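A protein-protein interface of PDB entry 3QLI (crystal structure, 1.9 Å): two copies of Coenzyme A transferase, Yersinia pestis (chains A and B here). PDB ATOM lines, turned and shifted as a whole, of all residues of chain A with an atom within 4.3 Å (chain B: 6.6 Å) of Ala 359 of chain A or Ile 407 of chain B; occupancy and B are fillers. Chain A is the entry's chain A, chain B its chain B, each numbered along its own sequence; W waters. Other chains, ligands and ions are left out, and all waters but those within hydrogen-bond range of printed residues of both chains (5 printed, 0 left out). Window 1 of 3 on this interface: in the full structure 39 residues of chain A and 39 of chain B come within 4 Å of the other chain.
Ala 359 of chain A touches just one residue of chain B: Ile 407 (3.3 Å).
Of the printed residues of chain A, Ile 407 of chain B touches Ser 126, Asn 127 and Ala 359.
Of the printed residues of chain A, Asp 408 of chain B touches Asn 127 (3.0 Å).
Of the printed residues of chain A, Arg 406 of chain B touches Tyr 123 (3.4 Å), Pro 125 (3.8 Å), Gln 356 (3.0 Å) and Tyr 357 (3.7 Å).
The nearest printed residue of chain A that does not touch Ile 407 of chain B is Ser 360 of chain A (4.1 Å).
Hydrophobic or aromatic side chains of chain A that line the printed part of chain B: Tyr 123, Pro 125, Tyr 357 and Ala 359.
Of the 11 printed residues of chain B, 4 touch a printed residue of chain A.
Hydrophobic or aromatic side chains of chain B that line the printed part of chain A: Ile 407.
Along chain B the printed residues that touch a printed residue of chain A span positions 406 to 429.
ND2 of Asn 127 of chain A sits at hydrogen-bond distance from O of Ile 407 of chain B, 3.1 Å away.
NH2 of Arg 406 of chain B lies within hydrogen-bond range of O of Gln 356 of chain A.
ND2 of Asn 127 of chain A is in hydrogen-bond range of OD1 of Asp 408 of chain B, 3.0 Å away.
The side-chain hydroxyl of Ser 358 of chain A sits at hydrogen-bond distance from the side-chain amide oxygen of Gln 356 of chain A (2.7 Å).
The backbone carbonyl oxygen of Thr 344 of chain B lies within hydrogen-bond range of the guanidinium group of Arg 429 of chain B.
OE1 of Gln 356 of chain A sits at hydrogen-bond distance from N of Ala 359 of chain A, 3.2 Å away.
The backbone carbonyl oxygen (O) of Ile 407 of chain B sits at hydrogen-bond distance from the side-chain amino group (NZ) of Lys 422 of chain B.
O of Ser 126 of chain A sits at hydrogen-bond distance from OG of Ser 360 of chain A (3.1 Å).
O of Arg 406 of chain B sits at hydrogen-bond distance from NH1 of Arg 429 of chain B, 2.8 Å away.
Tyr 123 of chain A touches Arg 406 of chain B (CE2 to NH2, 3.4 Å).
Pro 125 of chain A touches Arg 406 of chain B (CG to CD, 3.8 Å).
Arg 429 of chain B touches Pro 125 of chain A.
Ile 407 of chain B touches Ser 126 of chain A (CG2 to O, 3.4 Å).
Tyr 357 of chain A touches Arg 406 of chain B.
Ala 359 of chain A touches Ile 407 of chain B.
Water W1 lies within hydrogen-bond range of O of Pro 125 of chain A (2.6 Å) and NH2 of Arg 429 of chain B (3.5 Å).
Water W2 lies within hydrogen-bond range of O of Pro 125 of chain A (2.6 Å) and NH2 of Arg 429 of chain B (3.0 Å).
Water W5 lies within hydrogen-bond range of the side-chain amino group of Lys 422 of chain B (2.9 Å), the side-chain carboxylate of Asp 408 of chain B (3.0 Å) and the side-chain amide nitrogen of Asn 127 of chain A (3.3 Å).
Water W3 lies within hydrogen-bond range of the backbone carbonyl oxygen (O) of Gln 356 of chain A (2.9 Å), the guanidinium group (NE) of Arg 406 of chain B (3.1 Å) and the side-chain hydroxyl (OH) of Tyr 123 of chain A (3.2 Å).
Water W4 bridges the backbone NH (N) of Asn 127 of chain A and the side-chain amino group (NZ) of Lys 422 of chain B.
No position is printed for both chains.
Of the 9 pairs that touch across the chains among the printed residues, none has its exchanged pair printed and touching as well.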
ATOM      1  N   TYR A 123     -30.523  -1.988  12.615  1.00  0.00           N
ATOM      2  CA  TYR A 123     -29.987  -3.169  11.952  1.00  0.00           C
ATOM      3  C   TYR A 123     -30.653  -4.449  12.452  1.00  0.00           C
ATOM      4  O   TYR A 123     -30.772  -4.664  13.655  1.00  0.00           O
ATOM      5  CB  TYR A 123     -28.474  -3.242  12.181  1.00  0.00           C
ATOM      6  CG  TYR A 123     -27.804  -4.480  11.616  1.00  0.00           C
ATOM      7  CD1 TYR A 123     -27.752  -4.707  10.244  1.00  0.00           C
ATOM      8  CD2 TYR A 123     -27.204  -5.402  12.454  1.00  0.00           C
ATOM      9  CE1 TYR A 123     -27.135  -5.843   9.724  1.00  0.00           C
ATOM     10  CE2 TYR A 123     -26.579  -6.539  11.950  1.00  0.00           C
ATOM     11  CZ  TYR A 123     -26.545  -6.749  10.589  1.00  0.00           C
ATOM     12  OH  TYR A 123     -25.919  -7.870  10.097  1.00  0.00           O
ATOM     13  N   PRO A 125     -29.968  -8.293  12.371  1.00  0.00           N
ATOM     14  CA  PRO A 125     -28.938  -9.256  11.957  1.00  0.00           C
ATOM     15  C   PRO A 125     -29.563 -10.465  11.264  1.00  0.00           C
ATOM     16  O   PRO A 125     -30.600 -10.967  11.711  1.00  0.00           O
ATOM     17  CB  PRO A 125     -28.288  -9.674  13.287  1.00  0.00           C
ATOM     18  CG  PRO A 125     -28.645  -8.547  14.269  1.00  0.00           C
ATOM     19  CD  PRO A 125     -30.020  -8.115  13.836  1.00  0.00           C
ATOM     20  N   SER A 126     -28.942 -10.931  10.184  1.00  0.00           N
ATOM     21  CA  SER A 126     -29.458 -12.096   9.486  1.00  0.00           C
ATOM     22  C   SER A 126     -28.419 -12.631   8.527  1.00  0.00           C
ATOM     23  O   SER A 126     -27.400 -11.980   8.290  1.00  0.00           O
ATOM     24  CB  SER A 126     -30.714 -11.734   8.686  1.00  0.00           C
ATOM     25  OG  SER A 126     -30.369 -11.037   7.491  1.00  0.00           O
ATOM     26  N   ASN A 127     -28.688 -13.815   7.981  1.00  0.00           N
ATOM     27  CA  ASN A 127     -28.024 -14.272   6.766  1.00  0.00           C
ATOM     28  C   ASN A 127     -28.879 -13.960   5.532  1.00  0.00           C
ATOM     29  O   ASN A 127     -30.070 -14.296   5.481  1.00  0.00           O
ATOM     30  CB  ASN A 127     -27.766 -15.768   6.822  1.00  0.00           C
ATOM     31  CG  ASN A 127     -26.801 -16.139   7.903  1.00  0.00           C
ATOM     32  OD1 ASN A 127     -25.611 -15.878   7.789  1.00  0.00           O
ATOM     33  ND2 ASN A 127     -27.301 -16.756   8.958  1.00  0.00           N
ATOM     34  N   GLN A 356     -19.730  -4.671  12.678  1.00  0.00           N
ATOM     35  CA  GLN A 356     -19.748  -5.743  11.695  1.00  0.00           C
ATOM     36  C   GLN A 356     -21.180  -5.928  11.206  1.00  0.00           C
ATOM     37  O   GLN A 356     -21.977  -6.625  11.836  1.00  0.00           O
ATOM     38  CB  GLN A 356     -19.170  -7.033  12.304  1.00  0.00           C
ATOM     39  CG  GLN A 356     -19.010  -8.204  11.339  1.00  0.00           C
ATOM     40  CD  GLN A 356     -18.210  -7.841  10.095  1.00  0.00           C
ATOM     41  OE1 GLN A 356     -18.761  -7.765   8.998  1.00  0.00           O
ATOM     42  NE2 GLN A 356     -16.914  -7.606  10.266  1.00  0.00           N
ATOM     43  N   TYR A 357     -21.511  -5.253  10.108  1.00  0.00           N
ATOM     44  CA  TYR A 357     -22.815  -5.408   9.479  1.00  0.00           C
ATOM     45  C   TYR A 357     -22.680  -6.171   8.166  1.00  0.00           C
ATOM     46  O   TYR A 357     -23.671  -6.655   7.629  1.00  0.00           O
ATOM     47  CB  TYR A 357     -23.456  -4.046   9.197  1.00  0.00           C
ATOM     48  CG  TYR A 357     -23.571  -3.160  10.407  1.00  0.00           C
ATOM     49  CD1 TYR A 357     -22.811  -2.000  10.516  1.00  0.00           C
ATOM     50  CD2 TYR A 357     -24.429  -3.486  11.449  1.00  0.00           C
ATOM     51  CE1 TYR A 357     -22.909  -1.187  11.623  1.00  0.00           C
ATOM     52  CE2 TYR A 357     -24.539  -2.678  12.564  1.00  0.00           C
ATOM     53  CZ  TYR A 357     -23.771  -1.534  12.648  1.00  0.00           C
ATOM     54  OH  TYR A 357     -23.879  -0.726  13.756  1.00  0.00           O
ATOM     55  N   SER A 358     -21.460  -6.274   7.642  1.00  0.00           N
ATOM     56  CA  SER A 358     -21.273  -6.886   6.323  1.00  0.00           C
ATOM     57  C   SER A 358     -21.384  -8.414   6.357  1.00  0.00           C
ATOM     58  O   SER A 358     -21.530  -9.051   5.317  1.00  0.00           O
ATOM     59  CB  SER A 358     -19.957  -6.436   5.662  1.00  0.00           C
ATOM     60  OG  SER A 358     -18.834  -6.895   6.391  1.00  0.00           O
ATOM     61  N   ALA A 359     -21.353  -8.997   7.551  1.00  0.00           N
ATOM     62  CA  ALA A 359     -21.460 -10.452   7.677  1.00  0.00           C
ATOM     63  C   ALA A 359     -22.836 -10.977   7.224  1.00  0.00           C
ATOM     64  O   ALA A 359     -23.030 -12.180   7.014  1.00  0.00           O
ATOM     65  CB  ALA A 359     -21.151 -10.879   9.108  1.00  0.00           C
ATOM     66  N   SER A 360     -23.785 -10.062   7.069  1.00  0.00           N
ATOM     67  CA  SER A 360     -25.108 -10.405   6.551  1.00  0.00           C
ATOM     68  C   SER A 360     -25.075 -10.759   5.071  1.00  0.00           C
ATOM     69  O   SER A 360     -25.980 -11.421   4.571  1.00  0.00           O
ATOM     70  CB  SER A 360     -26.068  -9.239   6.766  1.00  0.00           C
ATOM     71  OG  SER A 360     -26.361  -9.106   8.137  1.00  0.00           O
ATOM     72  N   GLY A 361     -24.043 -10.301   4.361  1.00  0.00           N
ATOM     73  CA  GLY A 361     -23.953 -10.538   2.928  1.00  0.00           C
ATOM     74  C   GLY A 361     -23.601 -11.982   2.599  1.00  0.00           C
ATOM     75  O   GLY A 361     -23.263 -12.760   3.485  1.00  0.00           O
ATOM     76  N   VAL A 402     -15.661 -10.614  12.673  1.00  0.00           N
ATOM     77  CA  VAL A 402     -15.122 -10.545  11.314  1.00  0.00           C
ATOM     78  C   VAL A 402     -16.182 -10.830  10.250  1.00  0.00           C
ATOM     79  O   VAL A 402     -17.314 -11.174  10.575  1.00  0.00           O
ATOM     80  CB  VAL A 402     -13.945 -11.511  11.158  1.00  0.00           C
ATOM     81  CG1 VAL A 402     -12.884 -11.203  12.205  1.00  0.00           C
ATOM     82  CG2 VAL A 402     -14.421 -12.960  11.279  1.00  0.00           C
ATOM     83  N   THR B 344     -25.446  -8.553  21.486  1.00  0.00           N
ATOM     84  CA  THR B 344     -25.805  -8.644  20.070  1.00  0.00           C
ATOM     85  C   THR B 344     -26.413 -10.015  19.764  1.00  0.00           C
ATOM     86  O   THR B 344     -27.002 -10.229  18.698  1.00  0.00           O
ATOM     87  CB  THR B 344     -24.593  -8.388  19.122  1.00  0.00           C
ATOM     88  OG1 THR B 344     -23.690  -9.507  19.150  1.00  0.00           O
ATOM     89  CG2 THR B 344     -23.846  -7.117  19.517  1.00  0.00           C
ATOM     90  N   GLY B 345     -26.259 -10.941  20.707  1.00  0.00           N
ATOM     91  CA  GLY B 345     -26.731 -12.301  20.526  1.00  0.00           C
ATOM     92  C   GLY B 345     -25.639 -13.252  20.040  1.00  0.00           C
ATOM     93  O   GLY B 345     -25.914 -14.416  19.730  1.00  0.00           O
ATOM     94  N   ALA B 346     -24.403 -12.765  19.957  1.00  0.00           N
ATOM     95  CA  ALA B 346     -23.279 -13.631  19.644  1.00  0.00           C
ATOM     96  C   ALA B 346     -22.887 -14.422  20.892  1.00  0.00           C
ATOM     97  O   ALA B 346     -23.141 -13.984  22.022  1.00  0.00           O
ATOM     98  CB  ALA B 346     -22.085 -12.815  19.105  1.00  0.00           C
ATOM     99  N   THR B 404     -20.310 -18.440  18.042  1.00  0.00           N
ATOM    100  CA  THR B 404     -21.515 -18.404  17.228  1.00  0.00           C
ATOM    101  C   THR B 404     -21.836 -16.948  16.941  1.00  0.00           C
ATOM    102  O   THR B 404     -22.083 -16.171  17.864  1.00  0.00           O
ATOM    103  CB  THR B 404     -22.727 -19.057  17.941  1.00  0.00           C
ATOM    104  OG1 THR B 404     -22.493 -20.461  18.101  1.00  0.00           O
ATOM    105  CG2 THR B 404     -24.003 -18.862  17.122  1.00  0.00           C
ATOM    106  N   PRO B 405     -21.809 -16.566  15.663  1.00  0.00           N
ATOM    107  CA  PRO B 405     -22.082 -15.189  15.238  1.00  0.00           C
ATOM    108  C   PRO B 405     -23.524 -14.788  15.497  1.00  0.00           C
ATOM    109  O   PRO B 405     -24.418 -15.641  15.490  1.00  0.00           O
ATOM    110  CB  PRO B 405     -21.836 -15.238  13.721  1.00  0.00           C
ATOM    111  CG  PRO B 405     -20.973 -16.427  13.502  1.00  0.00           C
ATOM    112  CD  PRO B 405     -21.373 -17.419  14.541  1.00  0.00           C
ATOM    113  N   ARG B 406     -23.766 -13.495  15.682  1.00  0.00           N
ATOM    114  CA  ARG B 406     -25.121 -13.034  15.978  1.00  0.00           C
ATOM    115  C   ARG B 406     -26.102 -13.286  14.828  1.00  0.00           C
ATOM    116  O   ARG B 406     -27.308 -13.416  15.042  1.00  0.00           O
ATOM    117  CB  ARG B 406     -25.112 -11.550  16.364  1.00  0.00           C
ATOM    118  CG  ARG B 406     -24.722 -10.625  15.223  1.00  0.00           C
ATOM    119  CD  ARG B 406     -25.123  -9.206  15.560  1.00  0.00           C
ATOM    120  NE  ARG B 406     -24.446  -8.246  14.698  1.00  0.00           N
ATOM    121  CZ  ARG B 406     -24.558  -6.932  14.837  1.00  0.00           C
ATOM    122  NH1 ARG B 406     -25.342  -6.437  15.793  1.00  0.00           N
ATOM    123  NH2 ARG B 406     -23.888  -6.125  14.030  1.00  0.00           N
ATOM    124  N   ILE B 407     -25.589 -13.372  13.603  1.00  0.00           N
ATOM    125  CA  ILE B 407     -26.452 -13.687  12.474  1.00  0.00           C
ATOM    126  C   ILE B 407     -26.950 -15.145  12.471  1.00  0.00           C
ATOM    127  O   ILE B 407     -27.874 -15.484  11.730  1.00  0.00           O
ATOM    128  CB  ILE B 407     -25.752 -13.372  11.146  1.00  0.00           C
ATOM    129  CG1 ILE B 407     -24.466 -14.181  11.013  1.00  0.00           C
ATOM    130  CG2 ILE B 407     -25.432 -11.884  11.072  1.00  0.00           C
ATOM    131  CD1 ILE B 407     -23.687 -13.886   9.732  1.00  0.00           C
ATOM    132  N   ASP B 408     -26.290 -16.001  13.248  1.00  0.00           N
ATOM    133  CA  ASP B 408     -26.637 -17.421  13.303  1.00  0.00           C
ATOM    134  C   ASP B 408     -27.390 -17.884  14.545  1.00  0.00           C
ATOM    135  O   ASP B 408     -28.014 -18.942  14.529  1.00  0.00           O
ATOM    136  CB  ASP B 408     -25.371 -18.269  13.174  1.00  0.00           C
ATOM    137  CG  ASP B 408     -24.747 -18.176  11.804  1.00  0.00           C
ATOM    138  OD1 ASP B 408     -25.496 -18.241  10.810  1.00  0.00           O
ATOM    139  OD2 ASP B 408     -23.511 -18.039  11.725  1.00  0.00           O
ATOM    140  N   THR B 409     -27.333 -17.107  15.617  1.00  0.00           N
ATOM    141  CA  THR B 409     -27.995 -17.519  16.847  1.00  0.00           C
ATOM    142  C   THR B 409     -29.501 -17.636  16.665  1.00  0.00           C
ATOM    143  O   THR B 409     -30.134 -16.788  16.041  1.00  0.00           O
ATOM    144  CB  THR B 409     -27.676 -16.565  18.008  1.00  0.00           C
ATOM    145  OG1 THR B 409     -26.258 -16.385  18.102  1.00  0.00           O
ATOM    146  CG2 THR B 409     -28.194 -17.135  19.317  1.00  0.00           C
ATOM    147  N   LYS B 422     -33.994 -14.821  16.110  1.00  0.00           N
ATOM    148  CA  LYS B 422     -34.146 -14.699  14.665  1.00  0.00           C
ATOM    149  C   LYS B 422     -35.198 -13.660  14.272  1.00  0.00           C
ATOM    150  O   LYS B 422     -36.368 -13.778  14.630  1.00  0.00           O
ATOM    151  CB  LYS B 422     -34.485 -16.052  14.039  1.00  0.00           C
ATOM    152  CG  LYS B 422     -33.319 -17.043  14.052  1.00  0.00           C
ATOM    153  CD  LYS B 422     -32.248 -16.669  13.012  1.00  0.00           C
ATOM    154  CE  LYS B 422     -31.189 -17.766  12.901  1.00  0.00           C
ATOM    155  NZ  LYS B 422     -30.172 -17.423  11.872  1.00  0.00           N
ATOM    156  N   ARG B 429     -33.127  -7.259  20.295  1.00  0.00           N
ATOM    157  CA  ARG B 429     -32.214  -8.255  20.839  1.00  0.00           C
ATOM    158  C   ARG B 429     -31.621  -7.830  22.174  1.00  0.00           C
ATOM    159  O   ARG B 429     -31.653  -8.598  23.136  1.00  0.00           O
ATOM    160  CB  ARG B 429     -31.086  -8.540  19.847  1.00  0.00           C
ATOM    161  CG  ARG B 429     -31.542  -9.339  18.631  1.00  0.00           C
ATOM    162  CD  ARG B 429     -30.350  -9.684  17.724  1.00  0.00           C
ATOM    163  NE  ARG B 429     -30.760 -10.598  16.666  1.00  0.00           N
ATOM    164  CZ  ARG B 429     -30.036 -11.627  16.247  1.00  0.00           C
ATOM    165  NH1 ARG B 429     -28.856 -11.867  16.799  1.00  0.00           N
ATOM    166  NH2 ARG B 429     -30.494 -12.411  15.274  1.00  0.00           N
HETATM  167  O   HOH W   1     -31.564 -13.368  12.128  1.00  0.00           O
HETATM  168  O   HOH W   2     -32.454 -10.942  13.599  1.00  0.00           O
HETATM  169  O   HOH W   3     -23.550  -9.109  11.863  1.00  0.00           O
HETATM  170  O   HOH W   4     -31.093 -15.236   9.467  1.00  0.00           O
HETATM  171  O   HOH W   5     -28.312 -19.342  10.829  1.00  0.00           O
